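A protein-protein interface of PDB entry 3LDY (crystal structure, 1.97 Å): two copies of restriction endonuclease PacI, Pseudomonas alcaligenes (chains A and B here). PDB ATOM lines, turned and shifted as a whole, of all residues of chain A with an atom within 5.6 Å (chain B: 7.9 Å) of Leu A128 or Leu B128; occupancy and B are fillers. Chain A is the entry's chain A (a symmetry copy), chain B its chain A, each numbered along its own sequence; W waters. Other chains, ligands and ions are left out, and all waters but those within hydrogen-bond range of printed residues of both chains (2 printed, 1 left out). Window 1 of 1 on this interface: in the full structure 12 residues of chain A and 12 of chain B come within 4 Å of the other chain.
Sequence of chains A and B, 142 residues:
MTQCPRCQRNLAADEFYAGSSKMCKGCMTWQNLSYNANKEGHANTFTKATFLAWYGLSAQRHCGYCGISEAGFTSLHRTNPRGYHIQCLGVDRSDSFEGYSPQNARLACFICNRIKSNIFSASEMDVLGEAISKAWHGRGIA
Among the printed residues, merely in contact across the chains: Leu A128 with Leu B128 (2.8 Å), Val A127 with Ala B131 (3.6 Å), Ala A131 with Val B127 (3.6 Å), Leu A128 with Ile B132 (3.7 Å), Ile A132 with Leu B128 (3.7 Å), Glu A124 with Ala B135 (3.8 Å), Leu A128 with Ala B131 (3.8 Å), Ala A131 with Leu B128 (3.8 Å), Ile A115 with Ile B115 (3.8 Å), Phe A120 with Ile B115 (3.8 Å), Ile A115 with Phe B120 (3.8 Å) and Phe A120 with Ala B135 (3.97 Å).
Hydrophobic or aromatic side chains of chain A that line the printed part of chain B: Ile A115, Phe A120, Val A127, Leu A128, Ala A131 and Ile A132. Printed residues of chain B that touch a printed residue of chain A: Ile B115, Phe B120, Val B127, Leu B128, Ala B131, Ile B132 and Ala B135.
Water W2 lies within hydrogen-bond range of O of Ala B131 (2.8 Å), O of Glu A124 (3.1 Å) and N of Ala B135 (3.4 Å). Water W1 lies within hydrogen-bond range of O of Ala A131 (2.8 Å) and O of Glu B124 (3.1 Å).
Ile A115 touches its own counterpart, Ile B115. Ile A115 touches Phe B120, and with the chains exchanged Phe A120 touches Ile B115. Val A127 touches Ala B131, and with the chains exchanged Ala A131 touches Val B127. Leu A128 touches Ala B131, and with the chains exchanged Ala A131 touches Leu B128. Of the 12 pairs that touch across the chains among the printed residues, 10 have their exchanged pair printed and touching as well.
Leu A128 touches just these residues of chain B: Leu B128, Ala B131 and Ile B132. Leu B128 touches just these residues of chain A: Leu A128 (2.8 Å), Ala A131 (3.8 Å) and Ile A132 (3.7 Å). Of the printed residues of chain A, Phe B120 touches Ile A115 (3.8 Å). Of the printed residues of chain B, Glu A124 touches Ala B135. Of the printed residues of chain B, Ile A115 touches Ile B115 and Phe B120. Of the printed residues of chain A, Val B127 touches Ala A131 (3.6 Å). Lys B134 touches none of the printed residues of chain A. Ala B122 touches none of the printed residues of chain A. The nearest residue of chain B that does not touch Leu A128 is Ile B115 (4.7 Å). The nearest printed residue of chain B that does not touch Ile A115 is Leu B128 (4.7 Å).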
ATOM      1  N   ILE A 115     -24.181   4.607  -2.237  1.00  0.00           N
ATOM      2  CA  ILE A 115     -23.604   5.878  -1.754  1.00  0.00           C
ATOM      3  C   ILE A 115     -23.193   6.809  -2.906  1.00  0.00           C
ATOM      4  O   ILE A 115     -23.560   8.002  -2.957  1.00  0.00           O
ATOM      5  CB  ILE A 115     -22.477   5.633  -0.739  1.00  0.00           C
ATOM      6  CG1 ILE A 115     -23.108   5.133   0.584  1.00  0.00           C
ATOM      7  CG2 ILE A 115     -21.619   6.922  -0.543  1.00  0.00           C
ATOM      8  CD1 ILE A 115     -22.155   4.471   1.462  1.00  0.00           C
ATOM      9  N   PHE A 120     -21.532  11.290  -6.872  1.00  0.00           N
ATOM     10  CA  PHE A 120     -20.067  11.385  -6.867  1.00  0.00           C
ATOM     11  C   PHE A 120     -19.417  10.778  -8.121  1.00  0.00           C
ATOM     12  O   PHE A 120     -19.901   9.757  -8.660  1.00  0.00           O
ATOM     13  CB  PHE A 120     -19.503  10.712  -5.588  1.00  0.00           C
ATOM     14  CG  PHE A 120     -20.011  11.346  -4.307  1.00  0.00           C
ATOM     15  CD1 PHE A 120     -20.960  10.705  -3.512  1.00  0.00           C
ATOM     16  CD2 PHE A 120     -19.587  12.618  -3.935  1.00  0.00           C
ATOM     17  CE1 PHE A 120     -21.446  11.302  -2.335  1.00  0.00           C
ATOM     18  CE2 PHE A 120     -20.081  13.230  -2.763  1.00  0.00           C
ATOM     19  CZ  PHE A 120     -21.012  12.572  -1.972  1.00  0.00           C
ATOM     20  N   GLU A 124     -13.943  10.895  -6.764  1.00  0.00           N
ATOM     21  CA  GLU A 124     -14.491  11.372  -5.493  1.00  0.00           C
ATOM     22  C   GLU A 124     -14.882  10.139  -4.646  1.00  0.00           C
ATOM     23  O   GLU A 124     -14.634  10.082  -3.431  1.00  0.00           O
ATOM     24  CB  GLU A 124     -15.719  12.287  -5.715  1.00  0.00           C
ATOM     25  CG  GLU A 124     -15.357  13.763  -6.036  1.00  0.00           C
ATOM     26  CD  GLU A 124     -16.491  14.619  -6.590  1.00  0.00           C
ATOM     27  OE1 GLU A 124     -17.639  14.103  -6.808  1.00  0.00           O
ATOM     28  OE2 GLU A 124     -16.229  15.852  -6.791  1.00  0.00           O
ATOM     29  N   MET A 125     -15.458   9.140  -5.306  1.00  0.00           N
ATOM     30  CA  MET A 125     -15.849   7.923  -4.600  1.00  0.00           C
ATOM     31  C   MET A 125     -14.624   7.102  -4.096  1.00  0.00           C
ATOM     32  O   MET A 125     -14.702   6.426  -3.052  1.00  0.00           O
ATOM     33  CB  MET A 125     -16.821   7.077  -5.425  1.00  0.00           C
ATOM     34  CG  MET A 125     -17.465   5.985  -4.553  1.00  0.00           C
ATOM     35  SD  MET A 125     -18.540   6.636  -3.240  1.00  0.00           S
ATOM     36  CE  MET A 125     -18.645   5.232  -2.101  1.00  0.00           C
ATOM     37  N   ASP A 126     -13.501   7.165  -4.800  1.00  0.00           N
ATOM     38  CA  ASP A 126     -12.289   6.498  -4.294  1.00  0.00           C
ATOM     39  C   ASP A 126     -11.948   6.979  -2.877  1.00  0.00           C
ATOM     40  O   ASP A 126     -11.580   6.180  -2.006  1.00  0.00           O
ATOM     41  CB  ASP A 126     -11.083   6.694  -5.236  1.00  0.00           C
ATOM     42  CG  ASP A 126     -11.154   5.803  -6.478  1.00  0.00           C
ATOM     43  OD1 ASP A 126     -11.905   4.807  -6.463  1.00  0.00           O
ATOM     44  OD2 ASP A 126     -10.463   6.100  -7.474  1.00  0.00           O
ATOM     45  N   VAL A 127     -12.073   8.287  -2.662  1.00  0.00           N
ATOM     46  CA  VAL A 127     -11.815   8.905  -1.366  1.00  0.00           C
ATOM     47  C   VAL A 127     -12.892   8.524  -0.331  1.00  0.00           C
ATOM     48  O   VAL A 127     -12.541   8.207   0.806  1.00  0.00           O
ATOM     49  CB  VAL A 127     -11.605  10.463  -1.487  1.00  0.00           C
ATOM     50  CG1 VAL A 127     -11.316  11.100  -0.122  1.00  0.00           C
ATOM     51  CG2 VAL A 127     -10.443  10.784  -2.445  1.00  0.00           C
ATOM     52  N   LEU A 128     -14.178   8.534  -0.709  1.00  0.00           N
ATOM     53  CA  LEU A 128     -15.232   7.998   0.189  1.00  0.00           C
ATOM     54  C   LEU A 128     -14.932   6.531   0.545  1.00  0.00           C
ATOM     55  O   LEU A 128     -15.072   6.105   1.708  1.00  0.00           O
ATOM     56  CB  LEU A 128     -16.628   8.079  -0.447  1.00  0.00           C
ATOM     57  CG  LEU A 128     -17.496   9.266  -0.069  1.00  0.00           C
ATOM     58  CD1 LEU A 128     -18.919   9.219  -0.567  1.00  0.00           C
ATOM     59  CD2 LEU A 128     -17.578   9.175   1.377  1.00  0.00           C
ATOM     60  N   GLY A 129     -14.513   5.765  -0.461  1.00  0.00           N
ATOM     61  CA  GLY A 129     -14.236   4.347  -0.279  1.00  0.00           C
ATOM     62  C   GLY A 129     -13.244   4.056   0.841  1.00  0.00           C
ATOM     63  O   GLY A 129     -13.450   3.130   1.642  1.00  0.00           O
ATOM     64  N   GLU A 130     -12.184   4.861   0.904  1.00  0.00           N
ATOM     65  CA  GLU A 130     -11.164   4.696   1.922  1.00  0.00           C
ATOM     66  C   GLU A 130     -11.748   4.911   3.327  1.00  0.00           C
ATOM     67  O   GLU A 130     -11.348   4.227   4.280  1.00  0.00           O
ATOM     68  CB  GLU A 130      -9.968   5.611   1.613  1.00  0.00           C
ATOM     69  CG  GLU A 130      -9.232   5.196   0.318  1.00  0.00           C
ATOM     70  CD  GLU A 130      -8.179   6.192  -0.161  1.00  0.00           C
ATOM     71  OE1 GLU A 130      -8.357   7.417   0.014  1.00  0.00           O
ATOM     72  OE2 GLU A 130      -7.172   5.739  -0.744  1.00  0.00           O
ATOM     73  N   ALA A 131     -12.710   5.835   3.442  1.00  0.00           N
ATOM     74  CA  ALA A 131     -13.367   6.110   4.722  1.00  0.00           C
ATOM     75  C   ALA A 131     -14.313   4.978   5.113  1.00  0.00           C
ATOM     76  O   ALA A 131     -14.373   4.580   6.277  1.00  0.00           O
ATOM     77  CB  ALA A 131     -14.108   7.436   4.681  1.00  0.00           C
ATOM     78  N   ILE A 132     -15.047   4.458   4.130  1.00  0.00           N
ATOM     79  CA  ILE A 132     -15.861   3.263   4.317  1.00  0.00           C
ATOM     80  C   ILE A 132     -15.027   2.047   4.785  1.00  0.00           C
ATOM     81  O   ILE A 132     -15.429   1.346   5.712  1.00  0.00           O
ATOM     82  CB  ILE A 132     -16.707   2.951   3.052  1.00  0.00           C
ATOM     83  CG1 ILE A 132     -17.701   4.092   2.834  1.00  0.00           C
ATOM     84  CG2 ILE A 132     -17.467   1.667   3.246  1.00  0.00           C
ATOM     85  CD1 ILE A 132     -18.443   4.108   1.425  1.00  0.00           C
ATOM     86  N   SER A 133     -13.856   1.846   4.181  1.00  0.00           N
ATOM     87  CA  SER A 133     -12.930   0.781   4.588  1.00  0.00           C
ATOM     88  C   SER A 133     -12.526   0.862   6.059  1.00  0.00           C
ATOM     89  O   SER A 133     -12.335  -0.156   6.715  1.00  0.00           O
ATOM     90  CB  SER A 133     -11.671   0.829   3.735  1.00  0.00           C
ATOM     91  OG  SER A 133     -10.938  -0.353   3.949  1.00  0.00           O
ATOM     92  N   TYR B  65     -21.510  16.512   9.545  1.00  0.00           N
ATOM     93  CA  TYR B  65     -20.602  15.545   8.932  1.00  0.00           C
ATOM     94  C   TYR B  65     -19.602  16.124   7.914  1.00  0.00           C
ATOM     95  O   TYR B  65     -18.374  15.953   8.083  1.00  0.00           O
ATOM     96  CB  TYR B  65     -21.407  14.393   8.327  1.00  0.00           C
ATOM     97  CG  TYR B  65     -22.161  13.658   9.399  1.00  0.00           C
ATOM     98  CD1 TYR B  65     -23.556  13.644   9.422  1.00  0.00           C
ATOM     99  CD2 TYR B  65     -21.467  13.014  10.443  1.00  0.00           C
ATOM    100  CE1 TYR B  65     -24.243  12.977  10.455  1.00  0.00           C
ATOM    101  CE2 TYR B  65     -22.149  12.356  11.467  1.00  0.00           C
ATOM    102  CZ  TYR B  65     -23.524  12.344  11.461  1.00  0.00           C
ATOM    103  OH  TYR B  65     -24.188  11.674  12.468  1.00  0.00           O
ATOM    104  N   CYS B  66     -20.101  16.795   6.869  1.00  0.00           N
ATOM    105  CA  CYS B  66     -19.237  17.243   5.764  1.00  0.00           C
ATOM    106  C   CYS B  66     -18.849  18.721   5.860  1.00  0.00           C
ATOM    107  O   CYS B  66     -17.963  19.170   5.135  1.00  0.00           O
ATOM    108  CB  CYS B  66     -19.842  16.933   4.377  1.00  0.00           C
ATOM    109  SG  CYS B  66     -21.272  17.978   3.862  1.00  0.00           S
ATOM    110  N   ILE B 111     -27.646  14.737   1.755  1.00  0.00           N
ATOM    111  CA  ILE B 111     -26.685  13.799   1.160  1.00  0.00           C
ATOM    112  C   ILE B 111     -26.028  12.945   2.253  1.00  0.00           C
ATOM    113  O   ILE B 111     -26.042  11.716   2.183  1.00  0.00           O
ATOM    114  CB  ILE B 111     -25.637  14.533   0.261  1.00  0.00           C
ATOM    115  CG1 ILE B 111     -26.288  14.858  -1.094  1.00  0.00           C
ATOM    116  CG2 ILE B 111     -24.400  13.654   0.046  1.00  0.00           C
ATOM    117  CD1 ILE B 111     -25.522  15.887  -1.942  1.00  0.00           C
ATOM    118  N   CYS B 112     -25.500  13.576   3.299  1.00  0.00           N
ATOM    119  CA  CYS B 112     -24.860  12.809   4.354  1.00  0.00           C
ATOM    120  C   CYS B 112     -25.863  11.962   5.124  1.00  0.00           C
ATOM    121  O   CYS B 112     -25.551  10.851   5.566  1.00  0.00           O
ATOM    122  CB  CYS B 112     -24.140  13.756   5.316  1.00  0.00           C
ATOM    123  SG  CYS B 112     -22.559  14.309   4.634  1.00  0.00           S
ATOM    124  N   ILE B 115     -26.593   8.918   3.102  1.00  0.00           N
ATOM    125  CA  ILE B 115     -25.413   8.032   3.103  1.00  0.00           C
ATOM    126  C   ILE B 115     -25.295   7.217   4.401  1.00  0.00           C
ATOM    127  O   ILE B 115     -25.142   5.976   4.392  1.00  0.00           O
ATOM    128  CB  ILE B 115     -24.131   8.803   2.751  1.00  0.00           C
ATOM    129  CG1 ILE B 115     -24.169   9.156   1.244  1.00  0.00           C
ATOM    130  CG2 ILE B 115     -22.864   7.978   3.140  1.00  0.00           C
ATOM    131  CD1 ILE B 115     -23.253  10.228   0.881  1.00  0.00           C
ATOM    132  N   LYS B 116     -25.416   7.927   5.508  1.00  0.00           N
ATOM    133  CA  LYS B 116     -25.337   7.356   6.830  1.00  0.00           C
ATOM    134  C   LYS B 116     -26.445   6.336   6.986  1.00  0.00           C
ATOM    135  O   LYS B 116     -26.217   5.259   7.544  1.00  0.00           O
ATOM    136  CB  LYS B 116     -25.472   8.462   7.901  1.00  0.00           C
ATOM    137  CG  LYS B 116     -25.544   7.971   9.337  1.00  0.00           C
ATOM    138  CD  LYS B 116     -25.453   9.191  10.363  1.00  0.00           C
ATOM    139  CE  LYS B 116     -25.644   8.745  11.789  1.00  0.00           C
ATOM    140  NZ  LYS B 116     -27.074   8.394  12.101  1.00  0.00           N
ATOM    141  N   ILE B 119     -26.894   2.567   8.506  1.00  0.00           N
ATOM    142  CA  ILE B 119     -25.776   1.671   8.269  1.00  0.00           C
ATOM    143  C   ILE B 119     -24.603   2.066   9.158  1.00  0.00           C
ATOM    144  O   ILE B 119     -24.068   1.219   9.838  1.00  0.00           O
ATOM    145  CB  ILE B 119     -25.299   1.751   6.797  1.00  0.00           C
ATOM    146  CG1 ILE B 119     -26.406   1.320   5.811  1.00  0.00           C
ATOM    147  CG2 ILE B 119     -24.070   0.943   6.595  1.00  0.00           C
ATOM    148  CD1 ILE B 119     -26.091   1.589   4.326  1.00  0.00           C
ATOM    149  N   PHE B 120     -24.201   3.338   9.126  1.00  0.00           N
ATOM    150  CA  PHE B 120     -23.018   3.821   9.850  1.00  0.00           C
ATOM    151  C   PHE B 120     -23.363   4.495  11.188  1.00  0.00           C
ATOM    152  O   PHE B 120     -24.401   5.183  11.307  1.00  0.00           O
ATOM    153  CB  PHE B 120     -22.213   4.793   8.948  1.00  0.00           C
ATOM    154  CG  PHE B 120     -21.735   4.153   7.659  1.00  0.00           C
ATOM    155  CD1 PHE B 120     -22.335   4.456   6.437  1.00  0.00           C
ATOM    156  CD2 PHE B 120     -20.727   3.194   7.681  1.00  0.00           C
ATOM    157  CE1 PHE B 120     -21.904   3.846   5.245  1.00  0.00           C
ATOM    158  CE2 PHE B 120     -20.299   2.567   6.491  1.00  0.00           C
ATOM    159  CZ  PHE B 120     -20.894   2.891   5.280  1.00  0.00           C
ATOM    160  N   SER B 121     -22.501   4.312  12.193  1.00  0.00           N
ATOM    161  CA  SER B 121     -22.614   5.072  13.428  1.00  0.00           C
ATOM    162  C   SER B 121     -22.141   6.507  13.169  1.00  0.00           C
ATOM    163  O   SER B 121     -21.445   6.776  12.195  1.00  0.00           O
ATOM    164  CB  SER B 121     -21.735   4.463  14.506  1.00  0.00           C
ATOM    165  OG  SER B 121     -20.393   4.731  14.173  1.00  0.00           O
ATOM    166  N   ALA B 122     -22.517   7.420  14.059  1.00  0.00           N
ATOM    167  CA  ALA B 122     -22.133   8.804  13.919  1.00  0.00           C
ATOM    168  C   ALA B 122     -20.612   8.954  13.827  1.00  0.00           C
ATOM    169  O   ALA B 122     -20.136   9.727  13.012  1.00  0.00           O
ATOM    170  CB  ALA B 122     -22.720   9.647  15.067  1.00  0.00           C
ATOM    171  N   SER B 123     -19.847   8.230  14.647  1.00  0.00           N
ATOM    172  CA  SER B 123     -18.385   8.332  14.534  1.00  0.00           C
ATOM    173  C   SER B 123     -17.808   7.757  13.239  1.00  0.00           C
ATOM    174  O   SER B 123     -16.852   8.325  12.721  1.00  0.00           O
ATOM    175  CB  SER B 123     -17.643   7.803  15.764  1.00  0.00           C
ATOM    176  OG  SER B 123     -18.012   6.485  16.043  1.00  0.00           O
ATOM    177  N   GLU B 124     -18.382   6.663  12.710  1.00  0.00           N
ATOM    178  CA  GLU B 124     -18.000   6.149  11.394  1.00  0.00           C
ATOM    179  C   GLU B 124     -18.370   7.217  10.338  1.00  0.00           C
ATOM    180  O   GLU B 124     -17.603   7.495   9.402  1.00  0.00           O
ATOM    181  CB  GLU B 124     -18.712   4.811  11.082  1.00  0.00           C
ATOM    182  CG  GLU B 124     -18.012   3.567  11.695  1.00  0.00           C
ATOM    183  CD  GLU B 124     -18.836   2.283  11.710  1.00  0.00           C
ATOM    184  OE1 GLU B 124     -20.039   2.285  11.281  1.00  0.00           O
ATOM    185  OE2 GLU B 124     -18.250   1.235  12.145  1.00  0.00           O
ATOM    186  N   MET B 125     -19.532   7.836  10.519  1.00  0.00           N
ATOM    187  CA  MET B 125     -19.965   8.873   9.586  1.00  0.00           C
ATOM    188  C   MET B 125     -19.081  10.154   9.662  1.00  0.00           C
ATOM    189  O   MET B 125     -18.893  10.855   8.649  1.00  0.00           O
ATOM    190  CB  MET B 125     -21.456   9.181   9.733  1.00  0.00           C
ATOM    191  CG  MET B 125     -21.956  10.022   8.545  1.00  0.00           C
ATOM    192  SD  MET B 125     -21.897   9.149   6.953  1.00  0.00           S
ATOM    193  CE  MET B 125     -21.967  10.514   5.765  1.00  0.00           C
ATOM    194  N   ASP B 126     -18.526  10.459  10.829  1.00  0.00           N
ATOM    195  CA  ASP B 126     -17.591  11.594  10.914  1.00  0.00           C
ATOM    196  C   ASP B 126     -16.444  11.439   9.907  1.00  0.00           C
ATOM    197  O   ASP B 126     -16.041  12.406   9.249  1.00  0.00           O
ATOM    198  CB  ASP B 126     -17.037  11.783  12.341  1.00  0.00           C
ATOM    199  CG  ASP B 126     -18.048  12.438  13.285  1.00  0.00           C
ATOM    200  OD1 ASP B 126     -19.013  13.058  12.797  1.00  0.00           O
ATOM    201  OD2 ASP B 126     -17.882  12.329  14.518  1.00  0.00           O
ATOM    202  N   VAL B 127     -15.928  10.217   9.800  1.00  0.00           N
ATOM    203  CA  VAL B 127     -14.850   9.890   8.872  1.00  0.00           C
ATOM    204  C   VAL B 127     -15.331   9.930   7.408  1.00  0.00           C
ATOM    205  O   VAL B 127     -14.624  10.479   6.562  1.00  0.00           O
ATOM    206  CB  VAL B 127     -14.139   8.533   9.247  1.00  0.00           C
ATOM    207  CG1 VAL B 127     -12.997   8.209   8.276  1.00  0.00           C
ATOM    208  CG2 VAL B 127     -13.578   8.589  10.679  1.00  0.00           C
ATOM    209  N   LEU B 128     -16.515   9.381   7.105  1.00  0.00           N
ATOM    210  CA  LEU B 128     -17.106   9.558   5.754  1.00  0.00           C
ATOM    211  C   LEU B 128     -17.268  11.055   5.436  1.00  0.00           C
ATOM    212  O   LEU B 128     -16.972  11.514   4.316  1.00  0.00           O
ATOM    213  CB  LEU B 128     -18.475   8.872   5.628  1.00  0.00           C
ATOM    214  CG  LEU B 128     -18.505   7.489   5.003  1.00  0.00           C
ATOM    215  CD1 LEU B 128     -19.877   6.925   4.731  1.00  0.00           C
ATOM    216  CD2 LEU B 128     -17.895   7.695   3.703  1.00  0.00           C
ATOM    217  N   GLY B 129     -17.733  11.810   6.429  1.00  0.00           N
ATOM    218  CA  GLY B 129     -17.979  13.235   6.256  1.00  0.00           C
ATOM    219  C   GLY B 129     -16.770  14.007   5.742  1.00  0.00           C
ATOM    220  O   GLY B 129     -16.898  14.860   4.850  1.00  0.00           O
ATOM    221  N   GLU B 130     -15.598  13.690   6.294  1.00  0.00           N
ATOM    222  CA  GLU B 130     -14.368  14.347   5.896  1.00  0.00           C
ATOM    223  C   GLU B 130     -14.051  14.073   4.417  1.00  0.00           C
ATOM    224  O   GLU B 130     -13.538  14.957   3.716  1.00  0.00           O
ATOM    225  CB  GLU B 130     -13.231  13.942   6.848  1.00  0.00           C
ATOM    226  CG  GLU B 130     -13.453  14.469   8.284  1.00  0.00           C
ATOM    227  CD  GLU B 130     -12.479  13.916   9.321  1.00  0.00           C
ATOM    228  OE1 GLU B 130     -12.055  12.745   9.214  1.00  0.00           O
ATOM    229  OE2 GLU B 130     -12.156  14.660  10.270  1.00  0.00           O
ATOM    230  N   ALA B 131     -14.385  12.867   3.945  1.00  0.00           N
ATOM    231  CA  ALA B 131     -14.164  12.495   2.545  1.00  0.00           C
ATOM    232  C   ALA B 131     -15.150  13.205   1.622  1.00  0.00           C
ATOM    233  O   ALA B 131     -14.781  13.671   0.543  1.00  0.00           O
ATOM    234  CB  ALA B 131     -14.245  10.990   2.360  1.00  0.00           C
ATOM    235  N   ILE B 132     -16.407  13.291   2.057  1.00  0.00           N
ATOM    236  CA  ILE B 132     -17.415  14.087   1.368  1.00  0.00           C
ATOM    237  C   ILE B 132     -17.008  15.574   1.241  1.00  0.00           C
ATOM    238  O   ILE B 132     -17.140  16.159   0.167  1.00  0.00           O
ATOM    239  CB  ILE B 132     -18.816  13.908   2.014  1.00  0.00           C
ATOM    240  CG1 ILE B 132     -19.254  12.454   1.837  1.00  0.00           C
ATOM    241  CG2 ILE B 132     -19.813  14.809   1.336  1.00  0.00           C
ATOM    242  CD1 ILE B 132     -20.518  12.000   2.694  1.00  0.00           C
ATOM    243  N   SER B 133     -16.469  16.150   2.317  1.00  0.00           N
ATOM    244  CA  SER B 133     -15.961  17.527   2.305  1.00  0.00           C
ATOM    245  C   SER B 133     -14.894  17.769   1.240  1.00  0.00           C
ATOM    246  O   SER B 133     -14.819  18.844   0.656  1.00  0.00           O
ATOM    247  CB  SER B 133     -15.379  17.882   3.665  1.00  0.00           C
ATOM    248  OG  SER B 133     -15.163  19.271   3.712  1.00  0.00           O
ATOM    249  N   LYS B 134     -14.056  16.767   0.991  1.00  0.00           N
ATOM    250  CA  LYS B 134     -13.045  16.882  -0.051  1.00  0.00           C
ATOM    251  C   LYS B 134     -13.709  16.958  -1.419  1.00  0.00           C
ATOM    252  O   LYS B 134     -13.301  17.770  -2.255  1.00  0.00           O
ATOM    253  CB  LYS B 134     -12.022  15.751   0.054  1.00  0.00           C
ATOM    254  CG  LYS B 134     -11.100  15.957   1.236  1.00  0.00           C
ATOM    255  CD  LYS B 134     -10.300  14.728   1.587  1.00  0.00           C
ATOM    256  CE  LYS B 134      -9.264  15.101   2.657  1.00  0.00           C
ATOM    257  NZ  LYS B 134      -9.139  14.030   3.684  1.00  0.00           N
ATOM    258  N   ALA B 135     -14.757  16.158  -1.641  1.00  0.00           N
ATOM    259  CA  ALA B 135     -15.539  16.300  -2.873  1.00  0.00           C
ATOM    260  C   ALA B 135     -16.002  17.767  -3.046  1.00  0.00           C
ATOM    261  O   ALA B 135     -15.736  18.392  -4.065  1.00  0.00           O
ATOM    262  CB  ALA B 135     -16.727  15.344  -2.909  1.00  0.00           C
HETATM  263  O   HOH W   1     -15.517   5.242   8.764  1.00  0.00           O
HETATM  264  O   HOH W   2     -14.196  12.887  -2.098  1.00  0.00           O
